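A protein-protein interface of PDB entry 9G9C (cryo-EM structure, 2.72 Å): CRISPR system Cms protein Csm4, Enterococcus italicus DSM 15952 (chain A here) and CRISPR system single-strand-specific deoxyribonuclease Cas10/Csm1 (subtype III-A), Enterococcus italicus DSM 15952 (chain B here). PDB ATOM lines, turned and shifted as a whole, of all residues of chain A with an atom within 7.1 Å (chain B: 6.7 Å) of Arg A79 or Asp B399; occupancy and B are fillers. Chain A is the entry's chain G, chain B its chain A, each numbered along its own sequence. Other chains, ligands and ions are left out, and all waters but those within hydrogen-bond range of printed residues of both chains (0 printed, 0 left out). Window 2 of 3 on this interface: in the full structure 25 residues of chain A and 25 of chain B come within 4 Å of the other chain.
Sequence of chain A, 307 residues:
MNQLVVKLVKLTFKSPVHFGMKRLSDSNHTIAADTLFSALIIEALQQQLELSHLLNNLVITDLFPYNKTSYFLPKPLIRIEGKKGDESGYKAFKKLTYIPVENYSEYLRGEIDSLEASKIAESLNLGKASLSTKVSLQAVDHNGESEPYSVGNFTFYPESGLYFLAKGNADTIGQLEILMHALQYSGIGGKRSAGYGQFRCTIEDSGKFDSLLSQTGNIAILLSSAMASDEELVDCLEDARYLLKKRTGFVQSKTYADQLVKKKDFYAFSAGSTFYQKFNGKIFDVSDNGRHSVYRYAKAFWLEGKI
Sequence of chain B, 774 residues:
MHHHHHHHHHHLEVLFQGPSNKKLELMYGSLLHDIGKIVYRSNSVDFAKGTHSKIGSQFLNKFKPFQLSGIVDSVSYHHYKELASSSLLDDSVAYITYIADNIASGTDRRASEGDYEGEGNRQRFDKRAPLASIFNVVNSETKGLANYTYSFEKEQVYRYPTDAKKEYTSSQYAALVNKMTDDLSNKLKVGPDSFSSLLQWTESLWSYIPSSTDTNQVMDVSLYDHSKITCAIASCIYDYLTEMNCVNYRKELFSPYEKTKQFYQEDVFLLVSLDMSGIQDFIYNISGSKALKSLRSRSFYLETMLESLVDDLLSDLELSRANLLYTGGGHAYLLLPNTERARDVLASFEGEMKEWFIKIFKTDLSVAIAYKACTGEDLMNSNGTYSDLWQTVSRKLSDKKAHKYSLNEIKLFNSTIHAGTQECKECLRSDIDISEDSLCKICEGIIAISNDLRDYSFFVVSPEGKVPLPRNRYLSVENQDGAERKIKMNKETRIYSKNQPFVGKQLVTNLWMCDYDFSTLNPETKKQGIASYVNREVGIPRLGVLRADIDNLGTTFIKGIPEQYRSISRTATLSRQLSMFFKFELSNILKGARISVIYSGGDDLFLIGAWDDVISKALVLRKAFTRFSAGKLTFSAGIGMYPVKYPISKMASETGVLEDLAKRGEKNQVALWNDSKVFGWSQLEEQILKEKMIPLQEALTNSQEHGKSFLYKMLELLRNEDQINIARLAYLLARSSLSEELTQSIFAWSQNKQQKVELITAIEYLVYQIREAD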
ATOM      1  N   PRO A  76      14.547   7.196  12.073  1.00  0.00           N
ATOM      2  CA  PRO A  76      14.569   6.672  10.703  1.00  0.00           C
ATOM      3  C   PRO A  76      15.938   6.113  10.349  1.00  0.00           C
ATOM      4  O   PRO A  76      16.970   6.605  10.808  1.00  0.00           O
ATOM      5  CB  PRO A  76      14.217   7.893   9.848  1.00  0.00           C
ATOM      6  CG  PRO A  76      14.587   9.062  10.689  1.00  0.00           C
ATOM      7  CD  PRO A  76      14.328   8.651  12.106  1.00  0.00           C
ATOM      8  N   LEU A  77      15.925   5.041   9.557  1.00  0.00           N
ATOM      9  CA  LEU A  77      17.194   4.421   9.115  1.00  0.00           C
ATOM     10  C   LEU A  77      17.624   5.141   7.835  1.00  0.00           C
ATOM     11  O   LEU A  77      17.393   4.594   6.743  1.00  0.00           O
ATOM     12  CB  LEU A  77      16.959   2.929   8.907  1.00  0.00           C
ATOM     13  CG  LEU A  77      16.399   2.187  10.124  1.00  0.00           C
ATOM     14  CD1 LEU A  77      16.304   0.698   9.882  1.00  0.00           C
ATOM     15  CD2 LEU A  77      17.224   2.476  11.363  1.00  0.00           C
ATOM     16  N   ILE A  78      18.176   6.346   7.978  1.00  0.00           N
ATOM     17  CA  ILE A  78      18.627   7.152   6.807  1.00  0.00           C
ATOM     18  C   ILE A  78      20.141   7.359   6.955  1.00  0.00           C
ATOM     19  O   ILE A  78      20.585   7.678   8.076  1.00  0.00           O
ATOM     20  CB  ILE A  78      17.866   8.487   6.741  1.00  0.00           C
ATOM     21  CG1 ILE A  78      17.857   9.201   8.092  1.00  0.00           C
ATOM     22  CG2 ILE A  78      16.447   8.281   6.212  1.00  0.00           C
ATOM     23  CD1 ILE A  78      17.562  10.686   8.003  1.00  0.00           C
ATOM     24  N   ARG A  79      20.908   7.132   5.886  1.00  0.00           N
ATOM     25  CA  ARG A  79      22.368   7.387   5.963  1.00  0.00           C
ATOM     26  C   ARG A  79      22.584   8.890   6.195  1.00  0.00           C
ATOM     27  O   ARG A  79      21.874   9.693   5.550  1.00  0.00           O
ATOM     28  CB  ARG A  79      23.078   6.906   4.694  1.00  0.00           C
ATOM     29  CG  ARG A  79      24.582   7.117   4.781  1.00  0.00           C
ATOM     30  CD  ARG A  79      25.317   6.697   3.524  1.00  0.00           C
ATOM     31  NE  ARG A  79      24.956   7.523   2.368  1.00  0.00           N
ATOM     32  CZ  ARG A  79      25.175   7.172   1.109  1.00  0.00           C
ATOM     33  NH1 ARG A  79      26.015   6.191   0.834  1.00  0.00           N
ATOM     34  NH2 ARG A  79      24.562   7.810   0.128  1.00  0.00           N
ATOM     35  N   ILE A  80      23.536   9.251   7.059  1.00  0.00           N
ATOM     36  CA  ILE A  80      23.768  10.689   7.397  1.00  0.00           C
ATOM     37  C   ILE A  80      25.282  10.945   7.436  1.00  0.00           C
ATOM     38  O   ILE A  80      25.961  10.209   8.186  1.00  0.00           O
ATOM     39  CB  ILE A  80      23.111  11.061   8.739  1.00  0.00           C
ATOM     40  CG1 ILE A  80      21.595  10.884   8.714  1.00  0.00           C
ATOM     41  CG2 ILE A  80      23.498  12.481   9.153  1.00  0.00           C
ATOM     42  CD1 ILE A  80      20.901  11.362   9.975  1.00  0.00           C
ATOM     43  N   LEU A 108      15.832  14.449   9.784  1.00  0.00           N
ATOM     44  CA  LEU A 108      15.743  14.032   8.387  1.00  0.00           C
ATOM     45  C   LEU A 108      16.594  14.918   7.486  1.00  0.00           C
ATOM     46  O   LEU A 108      17.256  14.423   6.566  1.00  0.00           O
ATOM     47  CB  LEU A 108      14.285  14.041   7.928  1.00  0.00           C
ATOM     48  CG  LEU A 108      13.411  12.891   8.429  1.00  0.00           C
ATOM     49  CD1 LEU A 108      11.995  13.024   7.896  1.00  0.00           C
ATOM     50  CD2 LEU A 108      14.012  11.555   8.029  1.00  0.00           C
ATOM     51  N   ILE A 219      10.806  10.274   0.819  1.00  0.00           N
ATOM     52  CA  ILE A 219      11.122   8.972   1.474  1.00  0.00           C
ATOM     53  C   ILE A 219       9.951   8.572   2.379  1.00  0.00           C
ATOM     54  O   ILE A 219       9.193   9.468   2.804  1.00  0.00           O
ATOM     55  CB  ILE A 219      12.459   9.034   2.239  1.00  0.00           C
ATOM     56  CG1 ILE A 219      13.132   7.661   2.297  1.00  0.00           C
ATOM     57  CG2 ILE A 219      12.286   9.641   3.631  1.00  0.00           C
ATOM     58  CD1 ILE A 219      14.454   7.652   3.039  1.00  0.00           C
ATOM     59  N   ALA A 240      16.311   0.235  -0.094  1.00  0.00           N
ATOM     60  CA  ALA A 240      15.603   0.323   1.202  1.00  0.00           C
ATOM     61  C   ALA A 240      16.593   0.150   2.346  1.00  0.00           C
ATOM     62  O   ALA A 240      17.439  -0.759   2.287  1.00  0.00           O
ATOM     63  CB  ALA A 240      14.509  -0.708   1.277  1.00  0.00           C
ATOM     64  N   ARG A 241      16.485   1.008   3.356  1.00  0.00           N
ATOM     65  CA  ARG A 241      17.346   0.832   4.545  1.00  0.00           C
ATOM     66  C   ARG A 241      16.429   0.445   5.706  1.00  0.00           C
ATOM     67  O   ARG A 241      15.473   1.194   5.979  1.00  0.00           O
ATOM     68  CB  ARG A 241      18.063   2.144   4.866  1.00  0.00           C
ATOM     69  CG  ARG A 241      18.485   3.008   3.687  1.00  0.00           C
ATOM     70  CD  ARG A 241      19.992   3.171   3.686  1.00  0.00           C
ATOM     71  NE  ARG A 241      20.487   3.488   5.030  1.00  0.00           N
ATOM     72  CZ  ARG A 241      21.767   3.546   5.365  1.00  0.00           C
ATOM     73  NH1 ARG A 241      22.699   3.293   4.464  1.00  0.00           N
ATOM     74  NH2 ARG A 241      22.112   3.839   6.606  1.00  0.00           N
ATOM     75  N   THR A 274      13.199   2.692   6.343  1.00  0.00           N
ATOM     76  CA  THR A 274      12.875   3.646   5.289  1.00  0.00           C
ATOM     77  C   THR A 274      12.844   2.943   3.969  1.00  0.00           C
ATOM     78  O   THR A 274      13.842   2.305   3.638  1.00  0.00           O
ATOM     79  CB  THR A 274      13.918   4.741   5.361  1.00  0.00           C
ATOM     80  OG1 THR A 274      15.134   4.010   5.282  1.00  0.00           O
ATOM     81  CG2 THR A 274      13.836   5.525   6.655  1.00  0.00           C
ATOM     82  N   ILE A 307      14.126  14.207   2.545  1.00  0.00           N
ATOM     83  CA  ILE A 307      15.555  14.148   2.829  1.00  0.00           C
ATOM     84  C   ILE A 307      16.336  14.766   1.676  1.00  0.00           C
ATOM     85  O   ILE A 307      15.755  15.357   0.767  1.00  0.00           O
ATOM     86  CB  ILE A 307      16.027  12.708   3.093  1.00  0.00           C
ATOM     87  CG1 ILE A 307      16.024  11.902   1.794  1.00  0.00           C
ATOM     88  CG2 ILE A 307      15.160  12.043   4.150  1.00  0.00           C
ATOM     89  CD1 ILE A 307      16.608  10.517   1.940  1.00  0.00           C
ATOM     90  N   SER B 394      34.262   1.976   5.543  1.00  0.00           N
ATOM     91  CA  SER B 394      33.273   1.934   6.610  1.00  0.00           C
ATOM     92  C   SER B 394      31.976   2.611   6.200  1.00  0.00           C
ATOM     93  O   SER B 394      30.927   2.330   6.788  1.00  0.00           O
ATOM     94  CB  SER B 394      33.831   2.585   7.875  1.00  0.00           C
ATOM     95  OG  SER B 394      34.957   1.873   8.359  1.00  0.00           O
ATOM     96  N   ARG B 395      32.026   3.502   5.207  1.00  0.00           N
ATOM     97  CA  ARG B 395      30.795   4.058   4.664  1.00  0.00           C
ATOM     98  C   ARG B 395      30.029   3.020   3.856  1.00  0.00           C
ATOM     99  O   ARG B 395      28.793   3.016   3.867  1.00  0.00           O
ATOM    100  CB  ARG B 395      31.103   5.284   3.805  1.00  0.00           C
ATOM    101  CG  ARG B 395      29.875   6.096   3.464  1.00  0.00           C
ATOM    102  CD  ARG B 395      29.828   7.363   4.290  1.00  0.00           C
ATOM    103  NE  ARG B 395      28.504   7.565   4.864  1.00  0.00           N
ATOM    104  CZ  ARG B 395      28.211   8.484   5.772  1.00  0.00           C
ATOM    105  NH1 ARG B 395      29.123   9.332   6.218  1.00  0.00           N
ATOM    106  NH2 ARG B 395      26.973   8.549   6.250  1.00  0.00           N
ATOM    107  N   LYS B 396      30.739   2.137   3.153  1.00  0.00           N
ATOM    108  CA  LYS B 396      30.070   1.084   2.402  1.00  0.00           C
ATOM    109  C   LYS B 396      29.577  -0.031   3.313  1.00  0.00           C
ATOM    110  O   LYS B 396      28.522  -0.619   3.051  1.00  0.00           O
ATOM    111  CB  LYS B 396      31.010   0.526   1.332  1.00  0.00           C
ATOM    112  CG  LYS B 396      31.436   1.546   0.287  1.00  0.00           C
ATOM    113  CD  LYS B 396      32.463   0.962  -0.671  1.00  0.00           C
ATOM    114  CE  LYS B 396      32.821   1.949  -1.769  1.00  0.00           C
ATOM    115  NZ  LYS B 396      31.653   2.264  -2.637  1.00  0.00           N
ATOM    116  N   LEU B 397      30.317  -0.321   4.386  1.00  0.00           N
ATOM    117  CA  LEU B 397      29.905  -1.362   5.322  1.00  0.00           C
ATOM    118  C   LEU B 397      28.541  -1.056   5.923  1.00  0.00           C
ATOM    119  O   LEU B 397      27.686  -1.944   6.026  1.00  0.00           O
ATOM    120  CB  LEU B 397      30.956  -1.512   6.423  1.00  0.00           C
ATOM    121  CG  LEU B 397      31.448  -2.919   6.752  1.00  0.00           C
ATOM    122  CD1 LEU B 397      31.918  -3.626   5.500  1.00  0.00           C
ATOM    123  CD2 LEU B 397      32.572  -2.843   7.768  1.00  0.00           C
ATOM    124  N   SER B 398      28.314   0.199   6.319  1.00  0.00           N
ATOM    125  CA  SER B 398      27.011   0.583   6.849  1.00  0.00           C
ATOM    126  C   SER B 398      25.911   0.416   5.810  1.00  0.00           C
ATOM    127  O   SER B 398      24.747   0.209   6.167  1.00  0.00           O
ATOM    128  CB  SER B 398      27.051   2.026   7.351  1.00  0.00           C
ATOM    129  OG  SER B 398      28.019   2.181   8.373  1.00  0.00           O
ATOM    130  N   ASP B 399      26.255   0.500   4.523  1.00  0.00           N
ATOM    131  CA  ASP B 399      25.270   0.257   3.478  1.00  0.00           C
ATOM    132  C   ASP B 399      25.024  -1.225   3.249  1.00  0.00           C
ATOM    133  O   ASP B 399      24.001  -1.587   2.659  1.00  0.00           O
ATOM    134  CB  ASP B 399      25.712   0.906   2.168  1.00  0.00           C
ATOM    135  CG  ASP B 399      25.867   2.403   2.285  1.00  0.00           C
ATOM    136  OD1 ASP B 399      25.878   2.914   3.424  1.00  0.00           O
ATOM    137  OD2 ASP B 399      25.978   3.068   1.235  1.00  0.00           O
ATOM    138  N   LYS B 400      25.936  -2.085   3.701  1.00  0.00           N
ATOM    139  CA  LYS B 400      25.734  -3.524   3.605  1.00  0.00           C
ATOM    140  C   LYS B 400      24.924  -4.074   4.769  1.00  0.00           C
ATOM    141  O   LYS B 400      24.513  -5.239   4.724  1.00  0.00           O
ATOM    142  CB  LYS B 400      27.084  -4.240   3.533  1.00  0.00           C
ATOM    143  CG  LYS B 400      27.892  -3.943   2.282  1.00  0.00           C
ATOM    144  CD  LYS B 400      27.265  -4.563   1.049  1.00  0.00           C
ATOM    145  CE  LYS B 400      28.209  -4.485  -0.139  1.00  0.00           C
ATOM    146  NZ  LYS B 400      28.609  -3.082  -0.432  1.00  0.00           N
ATOM    147  N   LYS B 401      24.692  -3.268   5.805  1.00  0.00           N
ATOM    148  CA  LYS B 401      23.891  -3.674   6.948  1.00  0.00           C
ATOM    149  C   LYS B 401      22.505  -3.053   6.957  1.00  0.00           C
ATOM    150  O   LYS B 401      21.663  -3.473   7.759  1.00  0.00           O
ATOM    151  CB  LYS B 401      24.616  -3.319   8.254  1.00  0.00           C
ATOM    152  CG  LYS B 401      26.020  -3.876   8.335  1.00  0.00           C
ATOM    153  CD  LYS B 401      26.632  -3.634   9.698  1.00  0.00           C
ATOM    154  CE  LYS B 401      28.047  -4.169   9.756  1.00  0.00           C
ATOM    155  NZ  LYS B 401      28.630  -4.034  11.117  1.00  0.00           N
ATOM    156  N   ALA B 402      22.243  -2.069   6.097  1.00  0.00           N
ATOM    157  CA  ALA B 402      20.896  -1.527   5.968  1.00  0.00           C
ATOM    158  C   ALA B 402      20.042  -2.420   5.075  1.00  0.00           C
ATOM    159  O   ALA B 402      19.012  -2.948   5.506  1.00  0.00           O
ATOM    160  CB  ALA B 402      20.953  -0.099   5.420  1.00  0.00           C
ATOM    161  N   HIS B 403      20.491  -2.644   3.837  1.00  0.00           N
ATOM    162  CA  HIS B 403      19.778  -3.587   2.934  1.00  0.00           C
ATOM    163  C   HIS B 403      20.480  -4.941   3.042  1.00  0.00           C
ATOM    164  O   HIS B 403      21.005  -5.440   2.029  1.00  0.00           O
ATOM    165  CB  HIS B 403      19.739  -3.042   1.506  1.00  0.00           C
ATOM    166  CG  HIS B 403      18.684  -3.652   0.648  1.00  0.00           C
ATOM    167  ND1 HIS B 403      18.296  -4.971   0.736  1.00  0.00           N
ATOM    168  CD2 HIS B 403      17.950  -3.117  -0.332  1.00  0.00           C
ATOM    169  CE1 HIS B 403      17.352  -5.209  -0.160  1.00  0.00           C
ATOM    170  NE2 HIS B 403      17.124  -4.095  -0.818  1.00  0.00           N
ATOM    171  N   LYS B 404      20.487  -5.520   4.240  1.00  0.00           N
ATOM    172  CA  LYS B 404      21.208  -6.794   4.488  1.00  0.00           C
ATOM    173  C   LYS B 404      20.650  -7.974   3.679  1.00  0.00           C
ATOM    174  O   LYS B 404      21.469  -8.788   3.222  1.00  0.00           O
ATOM    175  CB  LYS B 404      21.169  -7.091   5.990  1.00  0.00           C
ATOM    176  CG  LYS B 404      22.132  -8.156   6.477  1.00  0.00           C
ATOM    177  CD  LYS B 404      22.220  -8.152   7.997  1.00  0.00           C
ATOM    178  CE  LYS B 404      22.577  -6.798   8.514  1.00  0.00           C
ATOM    179  NZ  LYS B 404      22.729  -6.789   9.970  1.00  0.00           N
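The guanidinium group of Arg A79 is in salt-bridge range of the side-chain carboxylate of Asp B399, at 3.1 Å. The backbone carbonyl oxygen (O) of Ile A80 is in hydrogen-bond range of the guanidinium group (NH2) of Arg B395 (2.7 Å). OD1 of Asp B399 lies within salt-bridge range of NH1 of Arg A241 (3.4 Å).
The backbone NH (N) of Thr A274 sits at hydrogen-bond distance from the backbone carbonyl oxygen (O) of Arg A241, at 2.7 Å.
Arg A79 touches Arg B395 (CG to NH2, 3.2 Å). His B403 touches Ala A240. NE of Arg A241 touches CB of Ala B402, at 3.6 Å.
Asp B399 touches two residues of chain A. Of the printed residues of chain A, Arg B395 touches Arg A79 (3.2 Å) and Ile A80 (2.7 Å). Of the printed residues of chain A, His B403 touches Ala A240 (3.3 Å). Printed residues of chain B within 4 Å of Ala A240: His B403. Printed residues of chain A within 4 Å of Ala B402: Arg A241 (3.6 Å). The nearest residue of chain B that does not touch Arg A79 is Ser B398 (6.2 Å). The nearest residue of chain A that does not touch Asp B399 is Ala A240 (6.6 Å). The nearest printed residue of chain B that does not touch Arg A241 is Ser B398 (4.1 Å).
Along chain B the printed residues that touch a printed residue of chain A span positions 395 to 403. Of the 11 printed residues of chain A, 4 touch a printed residue of chain B. Printed residues of chain A that touch a printed residue of chain B: Arg A79, Ile A80, Ala A240 and Arg A241. Along chain A the printed residues that touch a printed residue of chain B span positions 79 to 241. Among the printed residues, Asp or Glu carboxylates within 4 Å of a Lys or Arg side-chain nitrogen of the other chain: Arg A79 with Asp B399 (3.1 Å) and Arg A241 with Asp B399 (3.4 Å).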
